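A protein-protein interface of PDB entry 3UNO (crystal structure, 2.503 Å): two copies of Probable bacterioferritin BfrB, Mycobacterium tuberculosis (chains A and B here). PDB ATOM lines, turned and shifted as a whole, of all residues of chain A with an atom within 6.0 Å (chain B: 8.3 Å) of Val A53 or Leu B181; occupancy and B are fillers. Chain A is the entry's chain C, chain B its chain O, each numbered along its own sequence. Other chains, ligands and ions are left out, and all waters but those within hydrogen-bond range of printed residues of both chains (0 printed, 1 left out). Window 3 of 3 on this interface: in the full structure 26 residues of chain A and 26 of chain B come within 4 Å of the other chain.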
ATOM      1  N   ALA A  26      -8.197 -24.881 -37.096  1.00  0.00           N
ATOM      2  CA  ALA A  26      -8.605 -24.907 -35.694  1.00  0.00           C
ATOM      3  C   ALA A  26      -7.524 -25.609 -34.847  1.00  0.00           C
ATOM      4  O   ALA A  26      -7.176 -25.139 -33.757  1.00  0.00           O
ATOM      5  CB  ALA A  26     -10.014 -25.591 -35.525  1.00  0.00           C
ATOM      6  N   PHE A  48      -6.703 -17.416 -28.012  1.00  0.00           N
ATOM      7  CA  PHE A  48      -6.495 -18.448 -29.032  1.00  0.00           C
ATOM      8  C   PHE A  48      -7.270 -19.775 -28.813  1.00  0.00           C
ATOM      9  O   PHE A  48      -7.695 -20.423 -29.790  1.00  0.00           O
ATOM     10  CB  PHE A  48      -4.989 -18.627 -29.324  1.00  0.00           C
ATOM     11  CG  PHE A  48      -4.484 -17.603 -30.290  1.00  0.00           C
ATOM     12  CD1 PHE A  48      -4.558 -17.835 -31.660  1.00  0.00           C
ATOM     13  CD2 PHE A  48      -4.044 -16.348 -29.848  1.00  0.00           C
ATOM     14  CE1 PHE A  48      -4.146 -16.850 -32.593  1.00  0.00           C
ATOM     15  CE2 PHE A  48      -3.638 -15.332 -30.784  1.00  0.00           C
ATOM     16  CZ  PHE A  48      -3.703 -15.592 -32.148  1.00  0.00           C
ATOM     17  N   TYR A  49      -7.500 -20.147 -27.539  1.00  0.00           N
ATOM     18  CA  TYR A  49      -8.424 -21.260 -27.240  1.00  0.00           C
ATOM     19  C   TYR A  49      -9.804 -20.928 -27.818  1.00  0.00           C
ATOM     20  O   TYR A  49     -10.514 -21.778 -28.390  1.00  0.00           O
ATOM     21  CB  TYR A  49      -8.526 -21.508 -25.723  1.00  0.00           C
ATOM     22  CG  TYR A  49      -7.312 -22.163 -25.098  1.00  0.00           C
ATOM     23  CD1 TYR A  49      -6.841 -23.389 -25.553  1.00  0.00           C
ATOM     24  CD2 TYR A  49      -6.625 -21.549 -24.082  1.00  0.00           C
ATOM     25  CE1 TYR A  49      -5.730 -24.009 -24.970  1.00  0.00           C
ATOM     26  CE2 TYR A  49      -5.521 -22.162 -23.478  1.00  0.00           C
ATOM     27  CZ  TYR A  49      -5.084 -23.381 -23.924  1.00  0.00           C
ATOM     28  OH  TYR A  49      -3.979 -23.971 -23.327  1.00  0.00           O
ATOM     29  N   SER A  50     -10.160 -19.660 -27.684  1.00  0.00           N
ATOM     30  CA  SER A  50     -11.459 -19.219 -28.084  1.00  0.00           C
ATOM     31  C   SER A  50     -11.518 -19.223 -29.592  1.00  0.00           C
ATOM     32  O   SER A  50     -12.519 -19.700 -30.207  1.00  0.00           O
ATOM     33  CB  SER A  50     -11.734 -17.817 -27.512  1.00  0.00           C
ATOM     34  OG  SER A  50     -13.006 -17.361 -27.937  1.00  0.00           O
ATOM     35  N   GLN A  51     -10.439 -18.737 -30.199  1.00  0.00           N
ATOM     36  CA  GLN A  51     -10.352 -18.712 -31.672  1.00  0.00           C
ATOM     37  C   GLN A  51     -10.362 -20.108 -32.291  1.00  0.00           C
ATOM     38  O   GLN A  51     -10.831 -20.281 -33.424  1.00  0.00           O
ATOM     39  CB  GLN A  51      -9.075 -17.982 -32.142  1.00  0.00           C
ATOM     40  CG  GLN A  51      -9.152 -16.478 -31.979  1.00  0.00           C
ATOM     41  CD  GLN A  51      -9.956 -15.808 -33.075  1.00  0.00           C
ATOM     42  OE1 GLN A  51     -10.118 -16.347 -34.170  1.00  0.00           O
ATOM     43  NE2 GLN A  51     -10.462 -14.620 -32.786  1.00  0.00           N
ATOM     44  N   ALA A  52      -9.841 -21.095 -31.564  1.00  0.00           N
ATOM     45  CA  ALA A  52      -9.834 -22.466 -32.071  1.00  0.00           C
ATOM     46  C   ALA A  52     -11.259 -23.007 -32.080  1.00  0.00           C
ATOM     47  O   ALA A  52     -11.670 -23.680 -33.026  1.00  0.00           O
ATOM     48  CB  ALA A  52      -8.912 -23.340 -31.257  1.00  0.00           C
ATOM     49  N   VAL A  53     -12.036 -22.647 -31.057  1.00  0.00           N
ATOM     50  CA  VAL A  53     -13.427 -23.076 -30.996  1.00  0.00           C
ATOM     51  C   VAL A  53     -14.216 -22.474 -32.169  1.00  0.00           C
ATOM     52  O   VAL A  53     -14.919 -23.203 -32.858  1.00  0.00           O
ATOM     53  CB  VAL A  53     -14.078 -22.728 -29.607  1.00  0.00           C
ATOM     54  CG1 VAL A  53     -15.607 -22.979 -29.626  1.00  0.00           C
ATOM     55  CG2 VAL A  53     -13.408 -23.549 -28.447  1.00  0.00           C
ATOM     56  N   GLU A  54     -14.081 -21.165 -32.389  1.00  0.00           N
ATOM     57  CA  GLU A  54     -14.675 -20.510 -33.533  1.00  0.00           C
ATOM     58  C   GLU A  54     -14.338 -21.101 -34.901  1.00  0.00           C
ATOM     59  O   GLU A  54     -15.237 -21.236 -35.728  1.00  0.00           O
ATOM     60  CB  GLU A  54     -14.395 -18.998 -33.553  1.00  0.00           C
ATOM     61  CG  GLU A  54     -15.576 -18.185 -33.037  1.00  0.00           C
ATOM     62  CD  GLU A  54     -16.892 -18.487 -33.789  1.00  0.00           C
ATOM     63  OE1 GLU A  54     -17.041 -18.043 -34.944  1.00  0.00           O
ATOM     64  OE2 GLU A  54     -17.786 -19.161 -33.229  1.00  0.00           O
ATOM     65  N   GLU A  55     -13.078 -21.459 -35.158  1.00  0.00           N
ATOM     66  CA  GLU A  55     -12.751 -22.143 -36.422  1.00  0.00           C
ATOM     67  C   GLU A  55     -13.460 -23.494 -36.520  1.00  0.00           C
ATOM     68  O   GLU A  55     -13.992 -23.859 -37.583  1.00  0.00           O
ATOM     69  CB  GLU A  55     -11.233 -22.326 -36.619  1.00  0.00           C
ATOM     70  CG  GLU A  55     -10.460 -21.018 -36.789  1.00  0.00           C
ATOM     71  CD  GLU A  55     -10.775 -20.267 -38.065  1.00  0.00           C
ATOM     72  OE1 GLU A  55     -10.783 -20.895 -39.139  1.00  0.00           O
ATOM     73  OE2 GLU A  55     -10.993 -19.033 -38.000  1.00  0.00           O
ATOM     74  N   ARG A  56     -13.458 -24.248 -35.424  1.00  0.00           N
ATOM     75  CA  ARG A  56     -14.254 -25.472 -35.381  1.00  0.00           C
ATOM     76  C   ARG A  56     -15.695 -25.182 -35.819  1.00  0.00           C
ATOM     77  O   ARG A  56     -16.270 -25.917 -36.647  1.00  0.00           O
ATOM     78  CB  ARG A  56     -14.199 -26.124 -33.997  1.00  0.00           C
ATOM     79  CG  ARG A  56     -14.724 -27.541 -33.937  1.00  0.00           C
ATOM     80  CD  ARG A  56     -14.828 -27.938 -32.459  1.00  0.00           C
ATOM     81  NE  ARG A  56     -15.148 -29.353 -32.218  1.00  0.00           N
ATOM     82  CZ  ARG A  56     -16.378 -29.822 -32.047  1.00  0.00           C
ATOM     83  NH1 ARG A  56     -17.381 -28.958 -32.105  1.00  0.00           N
ATOM     84  NH2 ARG A  56     -16.582 -31.136 -31.807  1.00  0.00           N
ATOM     85  N   ASN A  57     -16.256 -24.098 -35.295  1.00  0.00           N
ATOM     86  CA  ASN A  57     -17.613 -23.726 -35.643  1.00  0.00           C
ATOM     87  C   ASN A  57     -17.768 -23.484 -37.138  1.00  0.00           C
ATOM     88  O   ASN A  57     -18.806 -23.820 -37.748  1.00  0.00           O
ATOM     89  CB  ASN A  57     -18.089 -22.476 -34.863  1.00  0.00           C
ATOM     90  CG  ASN A  57     -18.385 -22.768 -33.389  1.00  0.00           C
ATOM     91  OD1 ASN A  57     -18.707 -23.901 -33.012  1.00  0.00           O
ATOM     92  ND2 ASN A  57     -18.307 -21.723 -32.548  1.00  0.00           N
ATOM     93  N   HIS A  58     -16.763 -22.845 -37.726  1.00  0.00           N
ATOM     94  CA  HIS A  58     -16.819 -22.533 -39.169  1.00  0.00           C
ATOM     95  C   HIS A  58     -16.871 -23.868 -39.928  1.00  0.00           C
ATOM     96  O   HIS A  58     -17.762 -24.112 -40.746  1.00  0.00           O
ATOM     97  CB  HIS A  58     -15.611 -21.681 -39.614  1.00  0.00           C
ATOM     98  CG  HIS A  58     -15.613 -20.285 -39.055  1.00  0.00           C
ATOM     99  ND1 HIS A  58     -14.522 -19.450 -39.153  1.00  0.00           N
ATOM    100  CD2 HIS A  58     -16.571 -19.587 -38.416  1.00  0.00           C
ATOM    101  CE1 HIS A  58     -14.804 -18.300 -38.564  1.00  0.00           C
ATOM    102  NE2 HIS A  58     -16.042 -18.349 -38.122  1.00  0.00           N
ATOM    103  N   LEU A 181     -20.501 -23.604 -30.605  1.00  0.00           N
ATOM    104  CA  LEU A 181     -19.905 -23.697 -29.265  1.00  0.00           C
ATOM    105  C   LEU A 181     -19.302 -22.392 -28.806  1.00  0.00           C
ATOM    106  O   LEU A 181     -18.769 -21.610 -29.626  1.00  0.00           O
ATOM    107  CB  LEU A 181     -18.784 -24.701 -29.225  1.00  0.00           C
ATOM    108  CG  LEU A 181     -19.104 -26.135 -29.557  1.00  0.00           C
ATOM    109  CD1 LEU A 181     -17.900 -26.958 -29.099  1.00  0.00           C
ATOM    110  CD2 LEU A 181     -20.390 -26.541 -28.847  1.00  0.00           C
ATOM    111  N   GLY A 182     -19.411 -22.161 -27.492  1.00  0.00           N
ATOM    112  CA  GLY A 182     -18.679 -21.110 -26.807  1.00  0.00           C
ATOM    113  C   GLY A 182     -17.527 -21.761 -26.053  1.00  0.00           C
ATOM    114  O   GLY A 182     -16.556 -21.108 -25.641  1.00  0.00           O
ATOM    115  N   SER B  50     -22.208 -33.781 -28.508  1.00  0.00           N
ATOM    116  CA  SER B  50     -21.849 -33.542 -27.117  1.00  0.00           C
ATOM    117  C   SER B  50     -20.688 -34.443 -26.654  1.00  0.00           C
ATOM    118  O   SER B  50     -19.787 -34.003 -25.926  1.00  0.00           O
ATOM    119  CB  SER B  50     -23.082 -33.793 -26.228  1.00  0.00           C
ATOM    120  OG  SER B  50     -22.734 -33.570 -24.870  1.00  0.00           O
ATOM    121  N   ALA B  52     -18.331 -35.653 -28.491  1.00  0.00           N
ATOM    122  CA  ALA B  52     -17.117 -35.305 -29.166  1.00  0.00           C
ATOM    123  C   ALA B  52     -16.474 -34.123 -28.409  1.00  0.00           C
ATOM    124  O   ALA B  52     -15.251 -34.086 -28.219  1.00  0.00           O
ATOM    125  CB  ALA B  52     -17.405 -34.948 -30.659  1.00  0.00           C
ATOM    126  N   VAL B  53     -17.302 -33.172 -27.968  1.00  0.00           N
ATOM    127  CA  VAL B  53     -16.832 -32.056 -27.163  1.00  0.00           C
ATOM    128  C   VAL B  53     -16.153 -32.590 -25.868  1.00  0.00           C
ATOM    129  O   VAL B  53     -15.100 -32.083 -25.426  1.00  0.00           O
ATOM    130  CB  VAL B  53     -18.008 -31.039 -26.859  1.00  0.00           C
ATOM    131  CG1 VAL B  53     -17.580 -30.002 -25.829  1.00  0.00           C
ATOM    132  CG2 VAL B  53     -18.449 -30.331 -28.119  1.00  0.00           C
ATOM    133  N   GLU B  54     -16.775 -33.575 -25.234  1.00  0.00           N
ATOM    134  CA  GLU B  54     -16.211 -34.115 -24.002  1.00  0.00           C
ATOM    135  C   GLU B  54     -14.883 -34.820 -24.245  1.00  0.00           C
ATOM    136  O   GLU B  54     -13.986 -34.710 -23.411  1.00  0.00           O
ATOM    137  CB  GLU B  54     -17.190 -35.056 -23.268  1.00  0.00           C
ATOM    138  CG  GLU B  54     -17.875 -34.408 -22.109  1.00  0.00           C
ATOM    139  CD  GLU B  54     -16.874 -33.951 -21.046  1.00  0.00           C
ATOM    140  OE1 GLU B  54     -16.275 -34.813 -20.343  1.00  0.00           O
ATOM    141  OE2 GLU B  54     -16.675 -32.716 -20.912  1.00  0.00           O
ATOM    142  N   GLU B  55     -14.738 -35.539 -25.366  1.00  0.00           N
ATOM    143  CA  GLU B  55     -13.443 -36.177 -25.633  1.00  0.00           C
ATOM    144  C   GLU B  55     -12.373 -35.117 -25.873  1.00  0.00           C
ATOM    145  O   GLU B  55     -11.227 -35.228 -25.415  1.00  0.00           O
ATOM    146  CB  GLU B  55     -13.468 -37.153 -26.807  1.00  0.00           C
ATOM    147  CG  GLU B  55     -14.352 -38.367 -26.567  1.00  0.00           C
ATOM    148  CD  GLU B  55     -13.782 -39.333 -25.530  1.00  0.00           C
ATOM    149  OE1 GLU B  55     -12.558 -39.621 -25.571  1.00  0.00           O
ATOM    150  OE2 GLU B  55     -14.576 -39.795 -24.669  1.00  0.00           O
ATOM    151  N   ARG B  56     -12.742 -34.091 -26.616  1.00  0.00           N
ATOM    152  CA  ARG B  56     -11.841 -32.956 -26.749  1.00  0.00           C
ATOM    153  C   ARG B  56     -11.428 -32.432 -25.358  1.00  0.00           C
ATOM    154  O   ARG B  56     -10.268 -32.070 -25.132  1.00  0.00           O
ATOM    155  CB  ARG B  56     -12.497 -31.850 -27.597  1.00  0.00           C
ATOM    156  CG  ARG B  56     -11.592 -30.682 -28.021  1.00  0.00           C
ATOM    157  CD  ARG B  56     -12.452 -29.589 -28.662  1.00  0.00           C
ATOM    158  NE  ARG B  56     -11.667 -28.501 -29.269  1.00  0.00           N
ATOM    159  CZ  ARG B  56     -11.264 -27.380 -28.638  1.00  0.00           C
ATOM    160  NH1 ARG B  56     -11.575 -27.216 -27.361  1.00  0.00           N
ATOM    161  NH2 ARG B  56     -10.541 -26.418 -29.276  1.00  0.00           N
ATOM    162  N   ASN B  57     -12.377 -32.407 -24.426  1.00  0.00           N
ATOM    163  CA  ASN B  57     -12.083 -31.981 -23.066  1.00  0.00           C
ATOM    164  C   ASN B  57     -11.076 -32.870 -22.385  1.00  0.00           C
ATOM    165  O   ASN B  57     -10.193 -32.384 -21.654  1.00  0.00           O
ATOM    166  CB  ASN B  57     -13.353 -31.867 -22.212  1.00  0.00           C
ATOM    167  CG  ASN B  57     -14.194 -30.648 -22.581  1.00  0.00           C
ATOM    168  OD1 ASN B  57     -13.664 -29.682 -23.108  1.00  0.00           O
ATOM    169  ND2 ASN B  57     -15.507 -30.681 -22.276  1.00  0.00           N
ATOM    170  N   HIS B  58     -11.219 -34.175 -22.605  1.00  0.00           N
ATOM    171  CA  HIS B  58     -10.305 -35.125 -21.980  1.00  0.00           C
ATOM    172  C   HIS B  58      -8.890 -34.852 -22.533  1.00  0.00           C
ATOM    173  O   HIS B  58      -7.943 -34.763 -21.784  1.00  0.00           O
ATOM    174  CB  HIS B  58     -10.729 -36.551 -22.271  1.00  0.00           C
ATOM    175  CG  HIS B  58     -12.023 -36.926 -21.635  1.00  0.00           C
ATOM    176  ND1 HIS B  58     -12.733 -38.058 -21.987  1.00  0.00           N
ATOM    177  CD2 HIS B  58     -12.747 -36.313 -20.671  1.00  0.00           C
ATOM    178  CE1 HIS B  58     -13.827 -38.125 -21.257  1.00  0.00           C
ATOM    179  NE2 HIS B  58     -13.861 -37.083 -20.443  1.00  0.00           N
ATOM    180  N   MET B  60      -7.719 -32.215 -23.638  1.00  0.00           N
ATOM    181  CA  MET B  60      -7.192 -30.959 -23.127  1.00  0.00           C
ATOM    182  C   MET B  60      -6.821 -31.081 -21.662  1.00  0.00           C
ATOM    183  O   MET B  60      -5.983 -30.311 -21.172  1.00  0.00           O
ATOM    184  CB  MET B  60      -8.159 -29.819 -23.391  1.00  0.00           C
ATOM    185  CG  MET B  60      -8.392 -29.480 -24.901  1.00  0.00           C
ATOM    186  SD  MET B  60      -6.836 -29.202 -25.790  1.00  0.00           S
ATOM    187  CE  MET B  60      -6.440 -27.475 -25.294  1.00  0.00           C
ATOM    188  N   MET B  61      -7.418 -32.046 -20.954  1.00  0.00           N
ATOM    189  CA  MET B  61      -6.988 -32.303 -19.557  1.00  0.00           C
ATOM    190  C   MET B  61      -5.597 -32.941 -19.505  1.00  0.00           C
ATOM    191  O   MET B  61      -4.797 -32.690 -18.581  1.00  0.00           O
ATOM    192  CB  MET B  61      -7.976 -33.154 -18.768  1.00  0.00           C
ATOM    193  CG  MET B  61      -9.331 -32.521 -18.678  1.00  0.00           C
ATOM    194  SD  MET B  61     -10.519 -33.739 -18.075  1.00  0.00           S
ATOM    195  CE  MET B  61     -12.106 -32.847 -18.223  1.00  0.00           C
ATOM    196  N   ALA B 176      -9.113 -28.618 -17.671  1.00  0.00           N
ATOM    197  CA  ALA B 176      -8.854 -28.781 -19.106  1.00  0.00           C
ATOM    198  C   ALA B 176      -8.185 -27.489 -19.648  1.00  0.00           C
ATOM    199  O   ALA B 176      -8.693 -26.371 -19.434  1.00  0.00           O
ATOM    200  CB  ALA B 176     -10.159 -29.065 -19.867  1.00  0.00           C
ATOM    201  N   ALA B 177      -7.067 -27.613 -20.364  1.00  0.00           N
ATOM    202  CA  ALA B 177      -6.407 -26.418 -20.926  1.00  0.00           C
ATOM    203  C   ALA B 177      -7.439 -25.717 -21.770  1.00  0.00           C
ATOM    204  O   ALA B 177      -8.098 -26.360 -22.615  1.00  0.00           O
ATOM    205  CB  ALA B 177      -5.244 -26.817 -21.808  1.00  0.00           C
ATOM    206  N   GLY B 178      -7.589 -24.418 -21.565  1.00  0.00           N
ATOM    207  CA  GLY B 178      -8.588 -23.675 -22.304  1.00  0.00           C
ATOM    208  C   GLY B 178      -9.992 -23.725 -21.706  1.00  0.00           C
ATOM    209  O   GLY B 178     -10.941 -23.144 -22.269  1.00  0.00           O
ATOM    210  N   GLY B 179     -10.150 -24.402 -20.570  1.00  0.00           N
ATOM    211  CA  GLY B 179     -11.473 -24.512 -19.950  1.00  0.00           C
ATOM    212  C   GLY B 179     -12.323 -25.651 -20.504  1.00  0.00           C
ATOM    213  O   GLY B 179     -12.176 -26.054 -21.654  1.00  0.00           O
ATOM    214  N   ARG B 180     -13.219 -26.184 -19.684  1.00  0.00           N
ATOM    215  CA  ARG B 180     -14.060 -27.309 -20.089  1.00  0.00           C
ATOM    216  C   ARG B 180     -15.234 -26.814 -20.917  1.00  0.00           C
ATOM    217  O   ARG B 180     -16.078 -26.072 -20.401  1.00  0.00           O
ATOM    218  CB  ARG B 180     -14.573 -28.039 -18.837  1.00  0.00           C
ATOM    219  CG  ARG B 180     -15.071 -29.436 -19.119  1.00  0.00           C
ATOM    220  CD  ARG B 180     -15.362 -30.213 -17.858  1.00  0.00           C
ATOM    221  NE  ARG B 180     -15.762 -31.588 -18.173  1.00  0.00           N
ATOM    222  CZ  ARG B 180     -16.217 -32.461 -17.276  1.00  0.00           C
ATOM    223  NH1 ARG B 180     -16.336 -32.110 -15.995  1.00  0.00           N
ATOM    224  NH2 ARG B 180     -16.558 -33.681 -17.659  1.00  0.00           N
ATOM    225  N   LEU B 181     -15.295 -27.194 -22.188  1.00  0.00           N
ATOM    226  CA  LEU B 181     -16.404 -26.754 -23.062  1.00  0.00           C
ATOM    227  C   LEU B 181     -17.710 -27.520 -22.891  1.00  0.00           C
ATOM    228  O   LEU B 181     -17.713 -28.740 -22.609  1.00  0.00           O
ATOM    229  CB  LEU B 181     -16.042 -26.913 -24.539  1.00  0.00           C
ATOM    230  CG  LEU B 181     -14.861 -26.166 -25.088  1.00  0.00           C
ATOM    231  CD1 LEU B 181     -14.993 -26.230 -26.574  1.00  0.00           C
ATOM    232  CD2 LEU B 181     -14.892 -24.758 -24.550  1.00  0.00           C
ATOM    233  N   GLY B 182     -18.815 -26.792 -23.062  1.00  0.00           N
ATOM    234  CA  GLY B 182     -20.139 -27.382 -23.157  1.00  0.00           C
ATOM    235  C   GLY B 182     -20.516 -27.293 -24.626  1.00  0.00           C
ATOM    236  O   GLY B 182     -21.418 -27.992 -25.107  1.00  0.00           O
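Val A53 touches Leu B181, and with the chains exchanged Leu A181 touches Val B53. Leu B181 touches its own counterpart, Leu A181.
Printed residues of chain B that touch a printed residue of chain A: Val B53, Met B60, Ala B177, Gly B178 and Leu B181. Along chain B the printed residues that touch a printed residue of chain A span positions 53 to 181. Hydrophobic or aromatic side chains of chain A within 4 Å of the printed part of chain B: Tyr A49, Val A53 and Leu A181.
Among the printed residues, pairs that only touch across the chains: Tyr A49 with Met B60, Tyr A49 with Ala B177, Tyr A49 with Gly B178, Val A53 with Leu B181, Leu A181 with Val B53 and Leu A181 with Leu B181.
Val A53 touches just one residue of chain B: Leu B181. Printed residues of chain A within 4 Å of Val B53: Leu A181. Arg B56 touches none of the printed residues of chain A. Of the printed residues of chain A, Met B60 touches Tyr A49. Of the printed residues of chain A, Ala B177 touches Tyr A49 (3.5 Å). Gly B182 touches none of the printed residues of chain A. The nearest residue of chain A that does not touch Leu B181 is Gly A182 (4.2 Å).
The backbone carbonyl oxygen (O) of Leu A181 lies within hydrogen-bond range of the side-chain amide nitrogen (ND2) of Asn A57. The backbone carbonyl oxygen of Val B53 lies close to the side-chain amide nitrogen of Asn B57, at 3.5 Å. The side-chain amide nitrogen (ND2) of Asn B57 is in hydrogen-bond range of the backbone carbonyl oxygen (O) of Leu B181. N of Ala B177 sits at hydrogen-bond distance from O of Met B60.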
